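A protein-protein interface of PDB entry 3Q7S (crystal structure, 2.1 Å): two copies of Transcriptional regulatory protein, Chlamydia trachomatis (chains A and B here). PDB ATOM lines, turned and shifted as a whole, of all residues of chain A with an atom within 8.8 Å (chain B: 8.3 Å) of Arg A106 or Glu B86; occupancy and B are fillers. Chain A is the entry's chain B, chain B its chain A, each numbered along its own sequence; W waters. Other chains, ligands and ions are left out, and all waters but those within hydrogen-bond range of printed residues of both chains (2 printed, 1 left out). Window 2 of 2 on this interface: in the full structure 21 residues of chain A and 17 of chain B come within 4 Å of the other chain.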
ATOM      1  N   LEU A  24      19.553  -0.645   4.951  1.00  0.00           N
ATOM      2  CA  LEU A  24      20.878  -1.078   5.287  1.00  0.00           C
ATOM      3  C   LEU A  24      21.688   0.092   5.835  1.00  0.00           C
ATOM      4  O   LEU A  24      22.410  -0.067   6.797  1.00  0.00           O
ATOM      5  CB  LEU A  24      21.554  -1.663   4.048  1.00  0.00           C
ATOM      6  CG  LEU A  24      22.968  -2.153   4.281  1.00  0.00           C
ATOM      7  CD1 LEU A  24      22.958  -3.323   5.284  1.00  0.00           C
ATOM      8  CD2 LEU A  24      23.586  -2.530   2.910  1.00  0.00           C
ATOM      9  N   GLN A  27      20.397   1.169   9.470  1.00  0.00           N
ATOM     10  CA  GLN A  27      20.605   0.134  10.477  1.00  0.00           C
ATOM     11  C   GLN A  27      22.090  -0.127  10.742  1.00  0.00           C
ATOM     12  O   GLN A  27      22.479  -0.473  11.834  1.00  0.00           O
ATOM     13  CB  GLN A  27      19.863  -1.123  10.062  1.00  0.00           C
ATOM     14  CG  GLN A  27      18.374  -0.892  10.113  1.00  0.00           C
ATOM     15  CD  GLN A  27      17.613  -2.150   9.890  1.00  0.00           C
ATOM     16  OE1 GLN A  27      18.067  -3.216  10.274  1.00  0.00           O
ATOM     17  NE2 GLN A  27      16.459  -2.051   9.235  1.00  0.00           N
ATOM     18  N   THR A  28      22.922   0.060   9.733  1.00  0.00           N
ATOM     19  CA  THR A  28      24.344  -0.131   9.894  1.00  0.00           C
ATOM     20  C   THR A  28      24.882   1.000  10.753  1.00  0.00           C
ATOM     21  O   THR A  28      25.685   0.775  11.683  1.00  0.00           O
ATOM     22  CB  THR A  28      25.064  -0.074   8.526  1.00  0.00           C
ATOM     23  OG1 THR A  28      24.665  -1.187   7.725  1.00  0.00           O
ATOM     24  CG2 THR A  28      26.603  -0.078   8.696  1.00  0.00           C
ATOM     25  N   LYS A  29      24.433   2.213  10.431  1.00  0.00           N
ATOM     26  CA  LYS A  29      24.975   3.431  11.033  1.00  0.00           C
ATOM     27  C   LYS A  29      24.655   3.423  12.488  1.00  0.00           C
ATOM     28  O   LYS A  29      25.436   3.829  13.332  1.00  0.00           O
ATOM     29  CB  LYS A  29      24.391   4.695  10.399  1.00  0.00           C
ATOM     30  CG  LYS A  29      24.836   5.933  11.164  1.00  0.00           C
ATOM     31  CD  LYS A  29      23.861   7.053  11.093  1.00  0.00           C
ATOM     32  CE  LYS A  29      24.088   7.820   9.896  1.00  0.00           C
ATOM     33  NZ  LYS A  29      24.308   9.202  10.335  1.00  0.00           N
ATOM     34  N   LEU A  31      24.635   0.906  14.281  1.00  0.00           N
ATOM     35  CA  LEU A  31      25.485  -0.028  15.030  1.00  0.00           C
ATOM     36  C   LEU A  31      26.884   0.498  15.283  1.00  0.00           C
ATOM     37  O   LEU A  31      27.585  -0.033  16.147  1.00  0.00           O
ATOM     38  CB  LEU A  31      25.587  -1.378  14.339  1.00  0.00           C
ATOM     39  CG  LEU A  31      24.228  -2.010  14.158  1.00  0.00           C
ATOM     40  CD1 LEU A  31      24.317  -3.283  13.356  1.00  0.00           C
ATOM     41  CD2 LEU A  31      23.600  -2.246  15.513  1.00  0.00           C
ATOM     42  N   LEU A  32      27.292   1.533  14.537  1.00  0.00           N
ATOM     43  CA  LEU A  32      28.643   2.068  14.641  1.00  0.00           C
ATOM     44  C   LEU A  32      28.642   3.262  15.597  1.00  0.00           C
ATOM     45  O   LEU A  32      27.822   4.147  15.474  1.00  0.00           O
ATOM     46  CB  LEU A  32      29.128   2.485  13.270  1.00  0.00           C
ATOM     47  CG  LEU A  32      29.343   1.345  12.275  1.00  0.00           C
ATOM     48  CD1 LEU A  32      29.479   1.924  10.886  1.00  0.00           C
ATOM     49  CD2 LEU A  32      30.561   0.532  12.630  1.00  0.00           C
ATOM     50  N   LEU A  99      31.809  -7.997  -0.680  1.00  0.00           N
ATOM     51  CA  LEU A  99      30.915  -8.907   0.001  1.00  0.00           C
ATOM     52  C   LEU A  99      29.842  -9.218  -0.974  1.00  0.00           C
ATOM     53  O   LEU A  99      29.464  -8.348  -1.744  1.00  0.00           O
ATOM     54  CB  LEU A  99      30.256  -8.238   1.208  1.00  0.00           C
ATOM     55  CG  LEU A  99      31.245  -7.906   2.300  1.00  0.00           C
ATOM     56  CD1 LEU A  99      30.571  -7.110   3.315  1.00  0.00           C
ATOM     57  CD2 LEU A  99      31.858  -9.196   2.907  1.00  0.00           C
ATOM     58  N   ILE A 103      23.901  -9.368   2.795  1.00  0.00           N
ATOM     59  CA  ILE A 103      24.735  -8.443   3.545  1.00  0.00           C
ATOM     60  C   ILE A 103      23.813  -7.772   4.586  1.00  0.00           C
ATOM     61  O   ILE A 103      22.927  -6.967   4.228  1.00  0.00           O
ATOM     62  CB  ILE A 103      25.375  -7.359   2.637  1.00  0.00           C
ATOM     63  CG1 ILE A 103      26.246  -7.960   1.514  1.00  0.00           C
ATOM     64  CG2 ILE A 103      26.181  -6.374   3.478  1.00  0.00           C
ATOM     65  CD1 ILE A 103      26.938  -6.894   0.540  1.00  0.00           C
ATOM     66  N   THR A 104      23.996  -8.114   5.864  1.00  0.00           N
ATOM     67  CA  THR A 104      23.171  -7.578   6.908  1.00  0.00           C
ATOM     68  C   THR A 104      23.865  -6.355   7.556  1.00  0.00           C
ATOM     69  O   THR A 104      25.077  -6.154   7.376  1.00  0.00           O
ATOM     70  CB  THR A 104      22.902  -8.660   7.951  1.00  0.00           C
ATOM     71  OG1 THR A 104      24.122  -8.976   8.635  1.00  0.00           O
ATOM     72  CG2 THR A 104      22.370  -9.937   7.249  1.00  0.00           C
ATOM     73  N   PRO A 105      23.103  -5.542   8.313  1.00  0.00           N
ATOM     74  CA  PRO A 105      23.760  -4.432   9.026  1.00  0.00           C
ATOM     75  C   PRO A 105      24.906  -4.880   9.968  1.00  0.00           C
ATOM     76  O   PRO A 105      25.941  -4.184  10.010  1.00  0.00           O
ATOM     77  CB  PRO A 105      22.612  -3.797   9.829  1.00  0.00           C
ATOM     78  CG  PRO A 105      21.384  -4.109   9.091  1.00  0.00           C
ATOM     79  CD  PRO A 105      21.630  -5.468   8.419  1.00  0.00           C
ATOM     80  N   ARG A 106      24.732  -6.010  10.681  1.00  0.00           N
ATOM     81  CA  ARG A 106      25.784  -6.502  11.559  1.00  0.00           C
ATOM     82  C   ARG A 106      27.029  -6.965  10.815  1.00  0.00           C
ATOM     83  O   ARG A 106      28.160  -6.754  11.282  1.00  0.00           O
ATOM     84  CB  ARG A 106      25.264  -7.614  12.463  1.00  0.00           C
ATOM     85  CG  ARG A 106      24.210  -7.092  13.500  1.00  0.00           C
ATOM     86  CD  ARG A 106      24.316  -7.938  14.725  1.00  0.00           C
ATOM     87  NE  ARG A 106      24.028  -9.304  14.373  1.00  0.00           N
ATOM     88  CZ  ARG A 106      24.483 -10.382  14.998  1.00  0.00           C
ATOM     89  NH1 ARG A 106      25.323 -10.277  16.028  1.00  0.00           N
ATOM     90  NH2 ARG A 106      24.087 -11.582  14.557  1.00  0.00           N
ATOM     91  N   ILE A 107      26.833  -7.608   9.678  1.00  0.00           N
ATOM     92  CA  ILE A 107      27.968  -7.946   8.824  1.00  0.00           C
ATOM     93  C   ILE A 107      28.662  -6.678   8.373  1.00  0.00           C
ATOM     94  O   ILE A 107      29.840  -6.494   8.700  1.00  0.00           O
ATOM     95  CB  ILE A 107      27.574  -8.863   7.643  1.00  0.00           C
ATOM     96  CG1 ILE A 107      27.280 -10.279   8.178  1.00  0.00           C
ATOM     97  CG2 ILE A 107      28.669  -8.938   6.598  1.00  0.00           C
ATOM     98  CD1 ILE A 107      26.664 -11.192   7.120  1.00  0.00           C
ATOM     99  N   LEU A 108      27.953  -5.775   7.701  1.00  0.00           N
ATOM    100  CA  LEU A 108      28.554  -4.512   7.258  1.00  0.00           C
ATOM    101  C   LEU A 108      29.312  -3.707   8.335  1.00  0.00           C
ATOM    102  O   LEU A 108      30.400  -3.222   8.076  1.00  0.00           O
ATOM    103  CB  LEU A 108      27.518  -3.598   6.632  1.00  0.00           C
ATOM    104  CG  LEU A 108      28.146  -2.484   5.749  1.00  0.00           C
ATOM    105  CD1 LEU A 108      29.222  -3.021   4.724  1.00  0.00           C
ATOM    106  CD2 LEU A 108      27.047  -1.755   5.052  1.00  0.00           C
ATOM    107  N   LYS A 109      28.724  -3.573   9.530  1.00  0.00           N
ATOM    108  CA  LYS A 109      29.321  -2.841  10.651  1.00  0.00           C
ATOM    109  C   LYS A 109      30.653  -3.506  10.992  1.00  0.00           C
ATOM    110  O   LYS A 109      31.635  -2.840  11.261  1.00  0.00           O
ATOM    111  CB  LYS A 109      28.366  -2.866  11.911  1.00  0.00           C
ATOM    112  CG  LYS A 109      29.097  -3.222  13.236  1.00  0.00           C
ATOM    113  CD  LYS A 109      28.232  -3.890  14.263  1.00  0.00           C
ATOM    114  CE  LYS A 109      28.811  -5.253  14.756  1.00  0.00           C
ATOM    115  NZ  LYS A 109      28.358  -6.451  13.968  1.00  0.00           N
ATOM    116  N   SER A 110      30.695  -4.833  10.988  1.00  0.00           N
ATOM    117  CA  SER A 110      31.929  -5.538  11.343  1.00  0.00           C
ATOM    118  C   SER A 110      32.984  -5.423  10.195  1.00  0.00           C
ATOM    119  O   SER A 110      34.194  -5.301  10.415  1.00  0.00           O
ATOM    120  CB  SER A 110      31.600  -6.986  11.722  1.00  0.00           C
ATOM    121  OG  SER A 110      31.115  -7.100  13.108  1.00  0.00           O
ATOM    122  N   ALA A 111      32.521  -5.458   8.980  1.00  0.00           N
ATOM    123  CA  ALA A 111      33.455  -5.383   7.828  1.00  0.00           C
ATOM    124  C   ALA A 111      34.114  -3.997   7.880  1.00  0.00           C
ATOM    125  O   ALA A 111      35.306  -3.878   7.924  1.00  0.00           O
ATOM    126  CB  ALA A 111      32.712  -5.584   6.543  1.00  0.00           C
ATOM    127  N   ILE A 112      33.290  -2.971   8.006  1.00  0.00           N
ATOM    128  CA  ILE A 112      33.738  -1.579   8.204  1.00  0.00           C
ATOM    129  C   ILE A 112      34.794  -1.421   9.302  1.00  0.00           C
ATOM    130  O   ILE A 112      35.854  -0.848   9.071  1.00  0.00           O
ATOM    131  CB  ILE A 112      32.540  -0.663   8.498  1.00  0.00           C
ATOM    132  CG1 ILE A 112      31.689  -0.526   7.230  1.00  0.00           C
ATOM    133  CG2 ILE A 112      32.976   0.745   9.016  1.00  0.00           C
ATOM    134  CD1 ILE A 112      30.439   0.258   7.439  1.00  0.00           C
ATOM    135  N   SER A 113      34.500  -1.939  10.488  1.00  0.00           N
ATOM    136  CA  SER A 113      35.433  -1.865  11.583  1.00  0.00           C
ATOM    137  C   SER A 113      36.688  -2.610  11.256  1.00  0.00           C
ATOM    138  O   SER A 113      37.744  -2.138  11.550  1.00  0.00           O
ATOM    139  CB  SER A 113      34.819  -2.441  12.859  1.00  0.00           C
ATOM    140  OG  SER A 113      33.519  -1.893  12.957  1.00  0.00           O
ATOM    141  N   TYR B  58      38.038 -22.460   6.696  1.00  0.00           N
ATOM    142  CA  TYR B  58      37.292 -22.271   7.954  1.00  0.00           C
ATOM    143  C   TYR B  58      37.196 -23.567   8.753  1.00  0.00           C
ATOM    144  O   TYR B  58      37.240 -23.596  10.001  1.00  0.00           O
ATOM    145  CB  TYR B  58      35.872 -21.777   7.642  1.00  0.00           C
ATOM    146  CG  TYR B  58      35.084 -21.391   8.864  1.00  0.00           C
ATOM    147  CD1 TYR B  58      35.457 -20.271   9.638  1.00  0.00           C
ATOM    148  CD2 TYR B  58      34.019 -22.189   9.327  1.00  0.00           C
ATOM    149  CE1 TYR B  58      34.784 -19.940  10.778  1.00  0.00           C
ATOM    150  CE2 TYR B  58      33.306 -21.844  10.479  1.00  0.00           C
ATOM    151  CZ  TYR B  58      33.676 -20.730  11.178  1.00  0.00           C
ATOM    152  OH  TYR B  58      33.004 -20.391  12.320  1.00  0.00           O
ATOM    153  N   ARG B  63      38.451 -22.336  16.433  1.00  0.00           N
ATOM    154  CA  ARG B  63      37.435 -21.398  16.813  1.00  0.00           C
ATOM    155  C   ARG B  63      37.913 -20.294  17.719  1.00  0.00           C
ATOM    156  O   ARG B  63      37.330 -19.197  17.752  1.00  0.00           O
ATOM    157  CB  ARG B  63      36.224 -22.134  17.383  1.00  0.00           C
ATOM    158  CG  ARG B  63      35.338 -22.556  16.227  1.00  0.00           C
ATOM    159  CD  ARG B  63      34.650 -21.287  15.599  1.00  0.00           C
ATOM    160  NE  ARG B  63      33.585 -20.888  16.511  1.00  0.00           N
ATOM    161  CZ  ARG B  63      32.458 -21.586  16.643  1.00  0.00           C
ATOM    162  NH1 ARG B  63      32.252 -22.693  15.893  1.00  0.00           N
ATOM    163  NH2 ARG B  63      31.542 -21.186  17.524  1.00  0.00           N
ATOM    164  N   PHE B  82      30.342 -21.608   3.118  1.00  0.00           N
ATOM    165  CA  PHE B  82      28.911 -21.319   3.257  1.00  0.00           C
ATOM    166  C   PHE B  82      28.693 -19.918   3.809  1.00  0.00           C
ATOM    167  O   PHE B  82      29.597 -19.382   4.460  1.00  0.00           O
ATOM    168  CB  PHE B  82      28.251 -22.336   4.244  1.00  0.00           C
ATOM    169  CG  PHE B  82      28.834 -22.274   5.635  1.00  0.00           C
ATOM    170  CD1 PHE B  82      28.440 -21.262   6.537  1.00  0.00           C
ATOM    171  CD2 PHE B  82      29.828 -23.155   6.011  1.00  0.00           C
ATOM    172  CE1 PHE B  82      28.969 -21.178   7.770  1.00  0.00           C
ATOM    173  CE2 PHE B  82      30.381 -23.099   7.245  1.00  0.00           C
ATOM    174  CZ  PHE B  82      29.977 -22.070   8.139  1.00  0.00           C
ATOM    175  N   PHE B  83      27.494 -19.351   3.580  1.00  0.00           N
ATOM    176  CA  PHE B  83      27.108 -18.092   4.182  1.00  0.00           C
ATOM    177  C   PHE B  83      26.344 -18.395   5.499  1.00  0.00           C
ATOM    178  O   PHE B  83      25.432 -19.197   5.482  1.00  0.00           O
ATOM    179  CB  PHE B  83      26.162 -17.244   3.275  1.00  0.00           C
ATOM    180  CG  PHE B  83      25.654 -16.025   3.986  1.00  0.00           C
ATOM    181  CD1 PHE B  83      26.512 -14.981   4.280  1.00  0.00           C
ATOM    182  CD2 PHE B  83      24.373 -15.980   4.513  1.00  0.00           C
ATOM    183  CE1 PHE B  83      26.081 -13.877   5.003  1.00  0.00           C
ATOM    184  CE2 PHE B  83      23.944 -14.872   5.243  1.00  0.00           C
ATOM    185  CZ  PHE B  83      24.798 -13.826   5.494  1.00  0.00           C
ATOM    186  N   ASP B  84      26.755 -17.769   6.598  1.00  0.00           N
ATOM    187  CA  ASP B  84      25.994 -17.732   7.858  1.00  0.00           C
ATOM    188  C   ASP B  84      26.361 -16.415   8.523  1.00  0.00           C
ATOM    189  O   ASP B  84      27.544 -16.076   8.620  1.00  0.00           O
ATOM    190  CB  ASP B  84      26.269 -18.924   8.783  1.00  0.00           C
ATOM    191  CG  ASP B  84      25.651 -18.761  10.153  1.00  0.00           C
ATOM    192  OD1 ASP B  84      24.402 -18.747  10.254  1.00  0.00           O
ATOM    193  OD2 ASP B  84      26.408 -18.640  11.143  1.00  0.00           O
ATOM    194  N   GLU B  85      25.340 -15.680   8.957  1.00  0.00           N
ATOM    195  CA  GLU B  85      25.528 -14.331   9.446  1.00  0.00           C
ATOM    196  C   GLU B  85      26.466 -14.254  10.637  1.00  0.00           C
ATOM    197  O   GLU B  85      27.374 -13.472  10.592  1.00  0.00           O
ATOM    198  CB  GLU B  85      24.179 -13.643   9.791  1.00  0.00           C
ATOM    199  CG  GLU B  85      24.408 -12.276  10.508  1.00  0.00           C
ATOM    200  CD  GLU B  85      23.137 -11.473  10.852  1.00  0.00           C
ATOM    201  OE1 GLU B  85      22.124 -12.072  11.226  1.00  0.00           O
ATOM    202  OE2 GLU B  85      23.164 -10.229  10.824  1.00  0.00           O
ATOM    203  N   GLU B  86      26.212 -15.014  11.718  1.00  0.00           N
ATOM    204  CA  GLU B  86      27.039 -14.957  12.910  1.00  0.00           C
ATOM    205  C   GLU B  86      28.445 -15.533  12.719  1.00  0.00           C
ATOM    206  O   GLU B  86      29.371 -15.104  13.376  1.00  0.00           O
ATOM    207  CB  GLU B  86      26.442 -15.791  14.042  1.00  0.00           C
ATOM    208  CG  GLU B  86      25.096 -15.440  14.429  1.00  0.00           C
ATOM    209  CD  GLU B  86      25.040 -14.205  15.270  1.00  0.00           C
ATOM    210  OE1 GLU B  86      26.056 -13.457  15.425  1.00  0.00           O
ATOM    211  OE2 GLU B  86      23.929 -13.968  15.773  1.00  0.00           O
ATOM    212  N   THR B  87      28.564 -16.581  11.915  1.00  0.00           N
ATOM    213  CA  THR B  87      29.848 -17.050  11.459  1.00  0.00           C
ATOM    214  C   THR B  87      30.668 -15.905  10.863  1.00  0.00           C
ATOM    215  O   THR B  87      31.817 -15.761  11.209  1.00  0.00           O
ATOM    216  CB  THR B  87      29.709 -18.154  10.427  1.00  0.00           C
ATOM    217  OG1 THR B  87      28.975 -19.208  10.997  1.00  0.00           O
ATOM    218  CG2 THR B  87      31.082 -18.692   9.910  1.00  0.00           C
ATOM    219  N   SER B  88      30.098 -15.155   9.930  1.00  0.00           N
ATOM    220  CA  SER B  88      30.768 -14.023   9.278  1.00  0.00           C
ATOM    221  C   SER B  88      31.095 -12.917  10.293  1.00  0.00           C
ATOM    222  O   SER B  88      32.246 -12.518  10.414  1.00  0.00           O
ATOM    223  CB  SER B  88      29.910 -13.476   8.099  1.00  0.00           C
ATOM    224  OG  SER B  88      29.820 -14.508   7.106  1.00  0.00           O
ATOM    225  N   VAL B  89      30.092 -12.470  11.054  1.00  0.00           N
ATOM    226  CA  VAL B  89      30.298 -11.457  12.084  1.00  0.00           C
ATOM    227  C   VAL B  89      31.472 -11.915  12.933  1.00  0.00           C
ATOM    228  O   VAL B  89      32.378 -11.165  13.182  1.00  0.00           O
ATOM    229  CB  VAL B  89      28.974 -11.172  12.967  1.00  0.00           C
ATOM    230  CG1 VAL B  89      29.279 -10.289  14.121  1.00  0.00           C
ATOM    231  CG2 VAL B  89      27.931 -10.544  12.084  1.00  0.00           C
ATOM    232  N   ASP B  90      31.463 -13.175  13.318  1.00  0.00           N
ATOM    233  CA  ASP B  90      32.492 -13.698  14.227  1.00  0.00           C
ATOM    234  C   ASP B  90      33.899 -13.710  13.635  1.00  0.00           C
ATOM    235  O   ASP B  90      34.839 -13.388  14.335  1.00  0.00           O
ATOM    236  CB  ASP B  90      32.107 -15.138  14.675  1.00  0.00           C
ATOM    237  CG  ASP B  90      33.156 -15.769  15.515  1.00  0.00           C
ATOM    238  OD1 ASP B  90      33.265 -15.327  16.668  1.00  0.00           O
ATOM    239  OD2 ASP B  90      33.854 -16.695  15.039  1.00  0.00           O
ATOM    240  N   LEU B  91      34.053 -14.118  12.346  1.00  0.00           N
ATOM    241  CA  LEU B  91      35.340 -14.023  11.698  1.00  0.00           C
ATOM    242  C   LEU B  91      35.806 -12.576  11.628  1.00  0.00           C
ATOM    243  O   LEU B  91      36.953 -12.298  11.892  1.00  0.00           O
ATOM    244  CB  LEU B  91      35.322 -14.603  10.292  1.00  0.00           C
ATOM    245  CG  LEU B  91      35.349 -16.115  10.156  1.00  0.00           C
ATOM    246  CD1 LEU B  91      35.031 -16.545   8.674  1.00  0.00           C
ATOM    247  CD2 LEU B  91      36.736 -16.620  10.642  1.00  0.00           C
ATOM    248  N   LEU B  92      34.932 -11.672  11.223  1.00  0.00           N
ATOM    249  CA  LEU B  92      35.321 -10.297  11.079  1.00  0.00           C
ATOM    250  C   LEU B  92      35.769  -9.714  12.433  1.00  0.00           C
ATOM    251  O   LEU B  92      36.795  -9.100  12.481  1.00  0.00           O
ATOM    252  CB  LEU B  92      34.227  -9.449  10.445  1.00  0.00           C
ATOM    253  CG  LEU B  92      33.848  -9.792   8.994  1.00  0.00           C
ATOM    254  CD1 LEU B  92      32.438  -9.161   8.685  1.00  0.00           C
ATOM    255  CD2 LEU B  92      34.969  -9.431   7.913  1.00  0.00           C
ATOM    256  N   ASP B  93      35.028  -9.969  13.529  1.00  0.00           N
ATOM    257  CA  ASP B  93      35.380  -9.393  14.851  1.00  0.00           C
ATOM    258  C   ASP B  93      36.655 -10.043  15.369  1.00  0.00           C
ATOM    259  O   ASP B  93      37.320  -9.443  16.141  1.00  0.00           O
ATOM    260  CB  ASP B  93      34.265  -9.614  15.882  1.00  0.00           C
ATOM    261  CG  ASP B  93      32.955  -8.833  15.545  1.00  0.00           C
ATOM    262  OD1 ASP B  93      32.931  -7.997  14.624  1.00  0.00           O
ATOM    263  OD2 ASP B  93      31.942  -9.009  16.246  1.00  0.00           O
ATOM    264  N   ARG B  94      36.974 -11.284  14.981  1.00  0.00           N
ATOM    265  CA  ARG B  94      38.239 -11.918  15.368  1.00  0.00           C
ATOM    266  C   ARG B  94      39.432 -11.457  14.482  1.00  0.00           C
ATOM    267  O   ARG B  94      40.581 -11.835  14.725  1.00  0.00           O
ATOM    268  CB  ARG B  94      38.110 -13.456  15.309  1.00  0.00           C
ATOM    269  CG  ARG B  94      37.249 -14.044  16.513  1.00  0.00           C
ATOM    270  CD  ARG B  94      36.720 -15.401  16.079  1.00  0.00           C
ATOM    271  NE  ARG B  94      37.795 -16.318  15.839  1.00  0.00           N
ATOM    272  CZ  ARG B  94      37.718 -17.461  15.170  1.00  0.00           C
ATOM    273  NH1 ARG B  94      36.589 -17.897  14.616  1.00  0.00           N
ATOM    274  NH2 ARG B  94      38.813 -18.185  15.103  1.00  0.00           N
ATOM    275  N   TYR B  98      37.626 -12.904   4.712  1.00  0.00           N
ATOM    276  CA  TYR B  98      37.352 -14.204   4.157  1.00  0.00           C
ATOM    277  C   TYR B  98      36.776 -14.131   2.735  1.00  0.00           C
ATOM    278  O   TYR B  98      36.287 -13.113   2.302  1.00  0.00           O
ATOM    279  CB  TYR B  98      36.350 -14.930   5.062  1.00  0.00           C
ATOM    280  CG  TYR B  98      35.074 -14.148   5.266  1.00  0.00           C
ATOM    281  CD1 TYR B  98      34.062 -14.181   4.308  1.00  0.00           C
ATOM    282  CD2 TYR B  98      34.878 -13.357   6.430  1.00  0.00           C
ATOM    283  CE1 TYR B  98      32.863 -13.438   4.500  1.00  0.00           C
ATOM    284  CE2 TYR B  98      33.716 -12.632   6.610  1.00  0.00           C
ATOM    285  CZ  TYR B  98      32.711 -12.672   5.655  1.00  0.00           C
ATOM    286  OH  TYR B  98      31.561 -11.933   5.833  1.00  0.00           O
HETATM  287  O   HOH W   1      22.153  -7.484  10.992  1.00  0.00           O
HETATM  288  O   HOH W   2      34.928  -6.083  13.453  1.00  0.00           O
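Printed residues of chain B within 4 Å of Arg A106: Glu B85 (3.7 Å), Glu B86 (2.7 Å) and Val B89 (3.9 Å).
Of the printed residues of chain B, Ser A110 touches Val B89 (3.8 Å), Leu B92 (3.8 Å) and Asp B93 (2.5 Å).
Printed residues of chain B within 4 Å of Ala A111: Leu B92 (3.7 Å).
Of the printed residues of chain A, Phe B83 touches Ile A107.
Glu B86 touches just one residue of chain A: Arg A106.
The nearest residue of chain B that does not touch Arg A106 is Leu B92 (5.6 Å).
The nearest printed residue of chain A that does not touch Phe B83 is Thr A104 (4.9 Å).
Water W1 lies within hydrogen-bond range of OE2 of Glu B85 (2.9 Å), N of Arg A106 (3.0 Å) and OG1 of Thr A104 (3.4 Å).
Water W2 bridges OD1 of Asp B93 and O of Ser A110.
The side-chain hydroxyl (OG1) of Thr A104 is in hydrogen-bond range of the backbone NH (N) of Ile A107, at 3.2 Å.
O of Arg A106 lies within hydrogen-bond range of NZ of Lys A109, at 2.7 Å.
O of Arg A106 sits close to OG of Ser A110.
The side-chain amino group of Lys A109 lies within hydrogen-bond range of the side-chain hydroxyl of Ser A110.
The side-chain hydroxyl of Ser A113 is in hydrogen-bond range of the backbone carbonyl oxygen of Lys A109 (2.7 Å).
Val B89 touches Arg A106.
Ile A107 touches Phe B83.
N of Ile A107 touches CG2 of Val B89 (3.95 Å).
Ile A107 touches Leu B92 (O to CD1, 3.7 Å).
Lys A109 touches Val B89 (NZ to CG1, 3.9 Å).
Val B89 touches Ser A110.
Ser A110 touches Leu B92.
Leu B92 touches Ala A111 (CD1 to N, 3.7 Å).
No position is printed for both chains.
Hydrophobic or aromatic side chains of chain B within 4 Å of the printed part of chain A: Phe B83, Val B89 and Leu B92.
Printed residues of chain A that touch a printed residue of chain B: Thr A104, Arg A106, Ile A107, Lys A109, Ser A110 and Ala A111.
Hydrophobic or aromatic side chains of chain A within 4 Å of the printed part of chain B: Ile A107.
Among the printed residues, 12 pairs touch across the chains.
The side-chain carboxylate (OE2) of Glu B85 lies within hydrogen-bond range of the side-chain hydroxyl (OG1) of Thr A104, 2.7 Å away.
The side-chain carboxylate (OE2) of Glu B85 lies within salt-bridge range of the guanidinium group (NE) of Arg A106 (3.8 Å).
NH2 of Arg A106 is in salt-bridge range of OE2 of Glu B86.
OD1 of Asp B93 lies within hydrogen-bond range of OG of Ser A110 (2.5 Å).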
